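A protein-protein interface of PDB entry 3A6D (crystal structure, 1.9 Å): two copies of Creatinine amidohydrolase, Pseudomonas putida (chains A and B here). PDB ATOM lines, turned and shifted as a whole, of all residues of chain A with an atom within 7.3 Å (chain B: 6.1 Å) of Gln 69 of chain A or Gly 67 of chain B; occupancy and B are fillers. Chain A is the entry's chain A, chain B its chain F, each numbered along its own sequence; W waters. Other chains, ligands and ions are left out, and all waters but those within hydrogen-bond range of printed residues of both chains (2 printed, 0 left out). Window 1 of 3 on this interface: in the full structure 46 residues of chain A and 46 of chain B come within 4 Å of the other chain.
The side-chain hydroxyl (OH) of Tyr 70 of chain A sits at hydrogen-bond distance from the backbone carbonyl oxygen (O) of Pro 66 of chain B (2.7 Å).
The backbone NH (N) of Leu 33 of chain A lies within hydrogen-bond range of the backbone carbonyl oxygen (O) of Gln 69 of chain A, 3.4 Å away.
The backbone carbonyl oxygen (O) of Leu 33 of chain A sits at hydrogen-bond distance from the backbone NH (N) of Thr 88 of chain A, 3.0 Å away.
The backbone carbonyl oxygen (O) of Gly 67 of chain A is in hydrogen-bond range of the side-chain amide nitrogen (NE2) of Gln 69 of chain A, at 2.9 Å.
The backbone carbonyl oxygen of Pro 29 of chain B is in hydrogen-bond range of the backbone NH of Leu 68 of chain B (2.9 Å).
The backbone carbonyl oxygen of Leu 68 of chain B lies within hydrogen-bond range of the backbone NH of Gly 31 of chain B, 2.9 Å away.
O of Gly 67 of chain B lies within hydrogen-bond range of NE2 of Gln 69 of chain B, at 2.9 Å.
Met 65 of chain B touches Leu 33 of chain A (CE to CD2, 3.7 Å).
Pro 66 of chain A touches Gln 69 of chain B (CB to CB, 3.8 Å).
O of Gly 67 of chain A touches CG of Gln 69 of chain B, 3.4 Å away.
Pro 66 of chain B touches Gln 69 of chain A (CB to CB, 3.8 Å).
Gln 69 of chain A touches Gly 67 of chain B (CG to O, 3.4 Å).
CG of Gln 69 of chain A touches NE2 of Gln 69 of chain B (3.9 Å).
OH of Tyr 70 of chain A touches CD1 of Leu 28 of chain B (3.7 Å).
Met 65 of chain B touches Tyr 70 of chain A (CB to OH, 3.5 Å).
CE1 of Tyr 70 of chain A touches CD2 of Leu 68 of chain B, 3.9 Å away.
Met 65 of chain B touches Thr 88 of chain A.
Of the printed residues of chain B, Leu 33 of chain A touches Met 65 and Pro 66.
Of the printed residues of chain B, Pro 66 of chain A touches Gln 69.
Gln 69 of chain A touches three residues of chain B.
Of the printed residues of chain B, Thr 88 of chain A touches Met 65 (3.7 Å).
Of chain A, only Gln 69 (3.4 Å) comes within 4 Å of Gly 67 of chain B.
Of the printed residues of chain A, Gln 69 of chain B touches Pro 66, Gly 67 and Gln 69.
Of the 11 printed residues of chain B, 6 touch a printed residue of chain A.
Hydrophobic or aromatic side chains of chain B that line the printed part of chain A: Leu 28, Met 65, Pro 66 and Leu 68.
Along chain B the printed residues that touch a printed residue of chain A span positions 28 to 69.
Of the 20 printed residues of chain A, 6 touch a printed residue of chain B.
Printed residues of chain A that touch a printed residue of chain B: Leu 33, Pro 66, Gly 67, Gln 69, Tyr 70 and Thr 88.
Hydrophobic or aromatic side chains of chain A within 4 Å of the printed part of chain B: Leu 33, Pro 66 and Tyr 70.
Among the printed residues, no Asp or Glu carboxylate lies within 4 Å of a Lys or Arg side-chain nitrogen of the other chain.
Pro 66 of chain A touches Gln 69 of chain B, and with the chains exchanged Gln 69 of chain A touches Pro 66 of chain B.
Gly 67 of chain A touches Gln 69 of chain B, and with the chains exchanged Gln 69 of chain A touches Gly 67 of chain B.
Gln 69 of chain B touches its own counterpart, Gln 69 of chain A.
Positions printed for both chains: 29, 30, 31, 46, 50, 66, 67, 68 and 69.
Of the 12 pairs that touch across the chains among the printed residues, 5 have their exchanged pair printed and touching as well.
Water W2 bridges the side-chain amide oxygen of Gln 69 of chain A (2.8 Å) and the backbone NH of Gly 67 of chain B (3.4 Å).
Water W1 lies within hydrogen-bond range of OE1 of Gln 69 of chain B and N of Gly 67 of chain A.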
ATOM      1  N   PRO A  29       0.656 -21.711 -28.253  1.00  0.00           N
ATOM      2  CA  PRO A  29      -0.794 -21.803 -28.055  1.00  0.00           C
ATOM      3  C   PRO A  29      -1.472 -20.856 -29.049  1.00  0.00           C
ATOM      4  O   PRO A  29      -1.025 -19.720 -29.213  1.00  0.00           O
ATOM      5  CB  PRO A  29      -0.989 -21.315 -26.614  1.00  0.00           C
ATOM      6  CG  PRO A  29       0.358 -21.472 -25.981  1.00  0.00           C
ATOM      7  CD  PRO A  29       1.303 -21.103 -27.079  1.00  0.00           C
ATOM      8  N   VAL A  30      -2.529 -21.311 -29.717  1.00  0.00           N
ATOM      9  CA  VAL A  30      -3.240 -20.459 -30.675  1.00  0.00           C
ATOM     10  C   VAL A  30      -4.702 -20.418 -30.259  1.00  0.00           C
ATOM     11  O   VAL A  30      -5.423 -21.409 -30.388  1.00  0.00           O
ATOM     12  CB  VAL A  30      -3.130 -21.008 -32.115  1.00  0.00           C
ATOM     13  CG1 VAL A  30      -3.727 -20.006 -33.106  1.00  0.00           C
ATOM     14  CG2 VAL A  30      -1.674 -21.289 -32.449  1.00  0.00           C
ATOM     15  N   GLY A  31      -5.139 -19.267 -29.760  1.00  0.00           N
ATOM     16  CA  GLY A  31      -6.508 -19.157 -29.291  1.00  0.00           C
ATOM     17  C   GLY A  31      -7.426 -18.193 -30.015  1.00  0.00           C
ATOM     18  O   GLY A  31      -7.453 -18.147 -31.248  1.00  0.00           O
ATOM     19  N   ALA A  32      -8.191 -17.437 -29.229  1.00  0.00           N
ATOM     20  CA  ALA A  32      -9.147 -16.464 -29.750  1.00  0.00           C
ATOM     21  C   ALA A  32      -9.839 -15.728 -28.609  1.00  0.00           C
ATOM     22  O   ALA A  32      -9.762 -16.144 -27.453  1.00  0.00           O
ATOM     23  CB  ALA A  32     -10.208 -17.175 -30.603  1.00  0.00           C
ATOM     24  N   LEU A  33     -10.490 -14.616 -28.946  1.00  0.00           N
ATOM     25  CA  LEU A  33     -11.278 -13.836 -27.995  1.00  0.00           C
ATOM     26  C   LEU A  33     -12.667 -14.063 -28.576  1.00  0.00           C
ATOM     27  O   LEU A  33     -12.995 -13.544 -29.651  1.00  0.00           O
ATOM     28  CB  LEU A  33     -10.921 -12.351 -28.050  1.00  0.00           C
ATOM     29  CG  LEU A  33     -11.759 -11.480 -27.111  1.00  0.00           C
ATOM     30  CD1 LEU A  33     -11.561 -11.931 -25.664  1.00  0.00           C
ATOM     31  CD2 LEU A  33     -11.353 -10.020 -27.282  1.00  0.00           C
ATOM     32  N   GLU A  34     -13.485 -14.839 -27.873  1.00  0.00           N
ATOM     33  CA  GLU A  34     -14.794 -15.205 -28.398  1.00  0.00           C
ATOM     34  C   GLU A  34     -15.835 -15.428 -27.304  1.00  0.00           C
ATOM     35  O   GLU A  34     -15.519 -15.921 -26.222  1.00  0.00           O
ATOM     36  CB  GLU A  34     -14.610 -16.494 -29.207  1.00  0.00           C
ATOM     37  CG  GLU A  34     -15.830 -17.063 -29.912  1.00  0.00           C
ATOM     38  CD  GLU A  34     -15.560 -18.478 -30.413  1.00  0.00           C
ATOM     39  OE1 GLU A  34     -16.097 -18.876 -31.466  1.00  0.00           O
ATOM     40  OE2 GLU A  34     -14.799 -19.194 -29.735  1.00  0.00           O
ATOM     41  N   MET A  42     -14.522 -14.648 -22.072  1.00  0.00           N
ATOM     42  CA  MET A  42     -14.205 -14.791 -23.486  1.00  0.00           C
ATOM     43  C   MET A  42     -12.789 -15.191 -23.912  1.00  0.00           C
ATOM     44  O   MET A  42     -12.557 -15.413 -25.100  1.00  0.00           O
ATOM     45  CB  MET A  42     -14.617 -13.508 -24.212  1.00  0.00           C
ATOM     46  CG  MET A  42     -16.078 -13.134 -23.998  1.00  0.00           C
ATOM     47  SD  MET A  42     -16.598 -11.728 -24.999  1.00  0.00           S
ATOM     48  CE  MET A  42     -16.007 -10.357 -24.004  1.00  0.00           C
ATOM     49  N   ASN A  43     -11.849 -15.302 -22.975  1.00  0.00           N
ATOM     50  CA  ASN A  43     -10.484 -15.680 -23.341  1.00  0.00           C
ATOM     51  C   ASN A  43     -10.185 -17.168 -23.144  1.00  0.00           C
ATOM     52  O   ASN A  43      -9.027 -17.591 -23.167  1.00  0.00           O
ATOM     53  CB  ASN A  43      -9.456 -14.821 -22.578  1.00  0.00           C
ATOM     54  CG  ASN A  43      -9.498 -15.026 -21.067  1.00  0.00           C
ATOM     55  OD1 ASN A  43      -8.782 -14.346 -20.325  1.00  0.00           O
ATOM     56  ND2 ASN A  43     -10.323 -15.954 -20.608  1.00  0.00           N
ATOM     57  N   ASP A  45     -10.334 -19.809 -25.046  1.00  0.00           N
ATOM     58  CA  ASP A  45      -9.501 -20.445 -26.061  1.00  0.00           C
ATOM     59  C   ASP A  45      -8.014 -20.158 -25.976  1.00  0.00           C
ATOM     60  O   ASP A  45      -7.218 -20.842 -26.617  1.00  0.00           O
ATOM     61  CB  ASP A  45     -10.036 -20.121 -27.456  1.00  0.00           C
ATOM     62  CG  ASP A  45     -11.379 -20.762 -27.704  1.00  0.00           C
ATOM     63  OD1 ASP A  45     -11.843 -21.478 -26.795  1.00  0.00           O
ATOM     64  OD2 ASP A  45     -11.964 -20.561 -28.782  1.00  0.00           O
ATOM     65  N   VAL A  46      -7.634 -19.145 -25.206  1.00  0.00           N
ATOM     66  CA  VAL A  46      -6.214 -18.853 -25.013  1.00  0.00           C
ATOM     67  C   VAL A  46      -5.802 -19.525 -23.704  1.00  0.00           C
ATOM     68  O   VAL A  46      -4.803 -20.240 -23.641  1.00  0.00           O
ATOM     69  CB  VAL A  46      -5.930 -17.335 -24.878  1.00  0.00           C
ATOM     70  CG1 VAL A  46      -4.467 -17.119 -24.478  1.00  0.00           C
ATOM     71  CG2 VAL A  46      -6.210 -16.635 -26.195  1.00  0.00           C
ATOM     72  N   LEU A  47      -6.593 -19.297 -22.661  1.00  0.00           N
ATOM     73  CA  LEU A  47      -6.308 -19.854 -21.341  1.00  0.00           C
ATOM     74  C   LEU A  47      -6.102 -21.362 -21.310  1.00  0.00           C
ATOM     75  O   LEU A  47      -5.123 -21.842 -20.743  1.00  0.00           O
ATOM     76  CB  LEU A  47      -7.425 -19.496 -20.355  1.00  0.00           C
ATOM     77  CG  LEU A  47      -7.539 -18.044 -19.886  1.00  0.00           C
ATOM     78  CD1 LEU A  47      -8.647 -17.938 -18.852  1.00  0.00           C
ATOM     79  CD2 LEU A  47      -6.211 -17.582 -19.290  1.00  0.00           C
ATOM     80  N   THR A  50      -2.981 -22.786 -23.295  1.00  0.00           N
ATOM     81  CA  THR A  50      -1.782 -22.288 -22.636  1.00  0.00           C
ATOM     82  C   THR A  50      -1.542 -23.092 -21.354  1.00  0.00           C
ATOM     83  O   THR A  50      -0.410 -23.455 -21.044  1.00  0.00           O
ATOM     84  CB  THR A  50      -1.909 -20.791 -22.277  1.00  0.00           C
ATOM     85  OG1 THR A  50      -2.168 -20.030 -23.466  1.00  0.00           O
ATOM     86  CG2 THR A  50      -0.616 -20.289 -21.637  1.00  0.00           C
ATOM     87  N   PRO A  66       4.653 -16.995 -26.365  1.00  0.00           N
ATOM     88  CA  PRO A  66       3.470 -16.192 -26.039  1.00  0.00           C
ATOM     89  C   PRO A  66       2.356 -16.655 -26.984  1.00  0.00           C
ATOM     90  O   PRO A  66       2.591 -16.841 -28.177  1.00  0.00           O
ATOM     91  CB  PRO A  66       3.931 -14.768 -26.340  1.00  0.00           C
ATOM     92  CG  PRO A  66       5.378 -14.809 -25.949  1.00  0.00           C
ATOM     93  CD  PRO A  66       5.844 -16.140 -26.524  1.00  0.00           C
ATOM     94  N   GLY A  67       1.152 -16.847 -26.462  1.00  0.00           N
ATOM     95  CA  GLY A  67       0.082 -17.339 -27.310  1.00  0.00           C
ATOM     96  C   GLY A  67      -0.580 -16.329 -28.226  1.00  0.00           C
ATOM     97  O   GLY A  67      -0.513 -15.124 -27.992  1.00  0.00           O
ATOM     98  N   LEU A  68      -1.201 -16.828 -29.291  1.00  0.00           N
ATOM     99  CA  LEU A  68      -1.925 -15.968 -30.213  1.00  0.00           C
ATOM    100  C   LEU A  68      -3.272 -15.731 -29.530  1.00  0.00           C
ATOM    101  O   LEU A  68      -4.021 -16.675 -29.246  1.00  0.00           O
ATOM    102  CB  LEU A  68      -2.090 -16.652 -31.576  1.00  0.00           C
ATOM    103  CG  LEU A  68      -0.766 -17.086 -32.227  1.00  0.00           C
ATOM    104  CD1 LEU A  68      -1.015 -17.461 -33.686  1.00  0.00           C
ATOM    105  CD2 LEU A  68       0.268 -15.961 -32.145  1.00  0.00           C
ATOM    106  N   GLN A  69      -3.553 -14.462 -29.247  1.00  0.00           N
ATOM    107  CA  GLN A  69      -4.757 -14.038 -28.541  1.00  0.00           C
ATOM    108  C   GLN A  69      -6.017 -13.906 -29.391  1.00  0.00           C
ATOM    109  O   GLN A  69      -7.139 -14.013 -28.876  1.00  0.00           O
ATOM    110  CB  GLN A  69      -4.483 -12.693 -27.855  1.00  0.00           C
ATOM    111  CG  GLN A  69      -3.145 -12.624 -27.100  1.00  0.00           C
ATOM    112  CD  GLN A  69      -3.140 -13.436 -25.811  1.00  0.00           C
ATOM    113  OE1 GLN A  69      -3.954 -13.206 -24.918  1.00  0.00           O
ATOM    114  NE2 GLN A  69      -2.210 -14.379 -25.706  1.00  0.00           N
ATOM    115  N   TYR A  70      -5.832 -13.657 -30.683  1.00  0.00           N
ATOM    116  CA  TYR A  70      -6.951 -13.487 -31.594  1.00  0.00           C
ATOM    117  C   TYR A  70      -6.895 -14.530 -32.696  1.00  0.00           C
ATOM    118  O   TYR A  70      -5.837 -14.762 -33.286  1.00  0.00           O
ATOM    119  CB  TYR A  70      -6.922 -12.076 -32.197  1.00  0.00           C
ATOM    120  CG  TYR A  70      -6.971 -10.971 -31.161  1.00  0.00           C
ATOM    121  CD1 TYR A  70      -5.804 -10.483 -30.571  1.00  0.00           C
ATOM    122  CD2 TYR A  70      -8.190 -10.424 -30.759  1.00  0.00           C
ATOM    123  CE1 TYR A  70      -5.854  -9.467 -29.604  1.00  0.00           C
ATOM    124  CE2 TYR A  70      -8.250  -9.420 -29.794  1.00  0.00           C
ATOM    125  CZ  TYR A  70      -7.081  -8.945 -29.223  1.00  0.00           C
ATOM    126  OH  TYR A  70      -7.148  -7.947 -28.275  1.00  0.00           O
ATOM    127  N   GLY A  71      -8.042 -15.149 -32.975  1.00  0.00           N
ATOM    128  CA  GLY A  71      -8.097 -16.181 -33.994  1.00  0.00           C
ATOM    129  C   GLY A  71      -9.068 -15.902 -35.125  1.00  0.00           C
ATOM    130  O   GLY A  71      -9.595 -14.791 -35.254  1.00  0.00           O
ATOM    131  N   THR A  88     -13.801 -11.068 -31.185  1.00  0.00           N
ATOM    132  CA  THR A  88     -12.936 -10.176 -31.962  1.00  0.00           C
ATOM    133  C   THR A  88     -12.045 -11.073 -32.813  1.00  0.00           C
ATOM    134  O   THR A  88     -11.061 -11.635 -32.324  1.00  0.00           O
ATOM    135  CB  THR A  88     -12.089  -9.319 -31.009  1.00  0.00           C
ATOM    136  OG1 THR A  88     -12.960  -8.645 -30.089  1.00  0.00           O
ATOM    137  CG2 THR A  88     -11.286  -8.283 -31.777  1.00  0.00           C
ATOM    138  N   LEU A  90      -9.805 -12.202 -36.478  1.00  0.00           N
ATOM    139  CA  LEU A  90      -8.880 -11.777 -37.516  1.00  0.00           C
ATOM    140  C   LEU A  90      -9.305 -12.364 -38.855  1.00  0.00           C
ATOM    141  O   LEU A  90     -10.049 -13.352 -38.912  1.00  0.00           O
ATOM    142  CB  LEU A  90      -7.461 -12.288 -37.218  1.00  0.00           C
ATOM    143  CG  LEU A  90      -6.833 -11.958 -35.863  1.00  0.00           C
ATOM    144  CD1 LEU A  90      -5.426 -12.559 -35.794  1.00  0.00           C
ATOM    145  CD2 LEU A  90      -6.790 -10.456 -35.678  1.00  0.00           C
ATOM    146  N   LEU B  28      -5.931  -1.177 -25.803  1.00  0.00           N
ATOM    147  CA  LEU B  28      -5.217  -2.302 -26.387  1.00  0.00           C
ATOM    148  C   LEU B  28      -3.708  -2.196 -26.216  1.00  0.00           C
ATOM    149  O   LEU B  28      -3.073  -1.339 -26.826  1.00  0.00           O
ATOM    150  CB  LEU B  28      -5.535  -2.412 -27.883  1.00  0.00           C
ATOM    151  CG  LEU B  28      -4.769  -3.492 -28.661  1.00  0.00           C
ATOM    152  CD1 LEU B  28      -5.166  -4.870 -28.138  1.00  0.00           C
ATOM    153  CD2 LEU B  28      -5.076  -3.382 -30.157  1.00  0.00           C
ATOM    154  N   PRO B  29      -3.118  -3.059 -25.375  1.00  0.00           N
ATOM    155  CA  PRO B  29      -1.668  -3.029 -25.167  1.00  0.00           C
ATOM    156  C   PRO B  29      -1.013  -3.625 -26.415  1.00  0.00           C
ATOM    157  O   PRO B  29      -1.503  -4.619 -26.957  1.00  0.00           O
ATOM    158  CB  PRO B  29      -1.465  -3.936 -23.947  1.00  0.00           C
ATOM    159  CG  PRO B  29      -2.810  -3.976 -23.287  1.00  0.00           C
ATOM    160  CD  PRO B  29      -3.757  -4.006 -24.448  1.00  0.00           C
ATOM    161  N   VAL B  30       0.074  -3.021 -26.883  1.00  0.00           N
ATOM    162  CA  VAL B  30       0.770  -3.528 -28.065  1.00  0.00           C
ATOM    163  C   VAL B  30       2.247  -3.653 -27.714  1.00  0.00           C
ATOM    164  O   VAL B  30       2.937  -2.647 -27.543  1.00  0.00           O
ATOM    165  CB  VAL B  30       0.602  -2.574 -29.265  1.00  0.00           C
ATOM    166  CG1 VAL B  30       1.226  -3.194 -30.511  1.00  0.00           C
ATOM    167  CG2 VAL B  30      -0.877  -2.284 -29.497  1.00  0.00           C
ATOM    168  N   GLY B  31       2.732  -4.887 -27.602  1.00  0.00           N
ATOM    169  CA  GLY B  31       4.120  -5.082 -27.223  1.00  0.00           C
ATOM    170  C   GLY B  31       5.012  -5.827 -28.192  1.00  0.00           C
ATOM    171  O   GLY B  31       5.015  -5.561 -29.395  1.00  0.00           O
ATOM    172  N   VAL B  46       5.230  -6.344 -23.314  1.00  0.00           N
ATOM    173  CA  VAL B  46       3.820  -6.708 -23.195  1.00  0.00           C
ATOM    174  C   VAL B  46       3.402  -6.449 -21.749  1.00  0.00           C
ATOM    175  O   VAL B  46       2.381  -5.808 -21.483  1.00  0.00           O
ATOM    176  CB  VAL B  46       3.571  -8.203 -23.514  1.00  0.00           C
ATOM    177  CG1 VAL B  46       2.133  -8.580 -23.144  1.00  0.00           C
ATOM    178  CG2 VAL B  46       3.811  -8.466 -24.990  1.00  0.00           C
ATOM    179  N   THR B  50       0.587  -3.465 -20.382  1.00  0.00           N
ATOM    180  CA  THR B  50      -0.602  -4.143 -19.878  1.00  0.00           C
ATOM    181  C   THR B  50      -0.830  -3.727 -18.422  1.00  0.00           C
ATOM    182  O   THR B  50      -1.954  -3.442 -18.022  1.00  0.00           O
ATOM    183  CB  THR B  50      -0.466  -5.688 -19.960  1.00  0.00           C
ATOM    184  OG1 THR B  50      -0.240  -6.081 -21.323  1.00  0.00           O
ATOM    185  CG2 THR B  50      -1.746  -6.363 -19.455  1.00  0.00           C
ATOM    186  N   MET B  65      -8.225  -4.863 -23.654  1.00  0.00           N
ATOM    187  CA  MET B  65      -8.257  -5.989 -24.592  1.00  0.00           C
ATOM    188  C   MET B  65      -6.992  -6.840 -24.477  1.00  0.00           C
ATOM    189  O   MET B  65      -5.966  -6.378 -23.984  1.00  0.00           O
ATOM    190  CB  MET B  65      -8.337  -5.475 -26.037  1.00  0.00           C
ATOM    191  CG  MET B  65      -9.601  -4.723 -26.407  1.00  0.00           C
ATOM    192  SD  MET B  65     -10.994  -5.825 -26.696  1.00  0.00           S
ATOM    193  CE  MET B  65     -10.502  -6.611 -28.278  1.00  0.00           C
ATOM    194  N   PRO B  66      -7.052  -8.104 -24.938  1.00  0.00           N
ATOM    195  CA  PRO B  66      -5.869  -8.972 -24.879  1.00  0.00           C
ATOM    196  C   PRO B  66      -4.755  -8.252 -25.643  1.00  0.00           C
ATOM    197  O   PRO B  66      -4.990  -7.728 -26.728  1.00  0.00           O
ATOM    198  CB  PRO B  66      -6.331 -10.233 -25.602  1.00  0.00           C
ATOM    199  CG  PRO B  66      -7.801 -10.300 -25.239  1.00  0.00           C
ATOM    200  CD  PRO B  66      -8.240  -8.848 -25.400  1.00  0.00           C
ATOM    201  N   GLY B  67      -3.549  -8.233 -25.089  1.00  0.00           N
ATOM    202  CA  GLY B  67      -2.465  -7.523 -25.747  1.00  0.00           C
ATOM    203  C   GLY B  67      -1.826  -8.203 -26.944  1.00  0.00           C
ATOM    204  O   GLY B  67      -1.884  -9.426 -27.088  1.00  0.00           O
ATOM    205  N   LEU B  68      -1.230  -7.405 -27.828  1.00  0.00           N
ATOM    206  CA  LEU B  68      -0.534  -7.973 -28.976  1.00  0.00           C
ATOM    207  C   LEU B  68       0.822  -8.387 -28.404  1.00  0.00           C
ATOM    208  O   LEU B  68       1.559  -7.562 -27.850  1.00  0.00           O
ATOM    209  CB  LEU B  68      -0.392  -6.937 -30.097  1.00  0.00           C
ATOM    210  CG  LEU B  68      -1.726  -6.388 -30.637  1.00  0.00           C
ATOM    211  CD1 LEU B  68      -1.481  -5.653 -31.957  1.00  0.00           C
ATOM    212  CD2 LEU B  68      -2.717  -7.519 -30.861  1.00  0.00           C
ATOM    213  N   GLN B  69       1.127  -9.675 -28.526  1.00  0.00           N
ATOM    214  CA  GLN B  69       2.342 -10.269 -27.972  1.00  0.00           C
ATOM    215  C   GLN B  69       3.591 -10.130 -28.834  1.00  0.00           C
ATOM    216  O   GLN B  69       4.711 -10.168 -28.318  1.00  0.00           O
ATOM    217  CB  GLN B  69       2.091 -11.758 -27.697  1.00  0.00           C
ATOM    218  CG  GLN B  69       0.741 -12.057 -27.032  1.00  0.00           C
ATOM    219  CD  GLN B  69       0.713 -11.704 -25.559  1.00  0.00           C
ATOM    220  OE1 GLN B  69       1.559 -12.153 -24.796  1.00  0.00           O
ATOM    221  NE2 GLN B  69      -0.268 -10.897 -25.151  1.00  0.00           N
HETATM  222  O   HOH W   1       1.151 -14.874 -23.855  1.00  0.00           O
HETATM  223  O   HOH W   2      -3.596 -11.003 -23.179  1.00  0.00           O
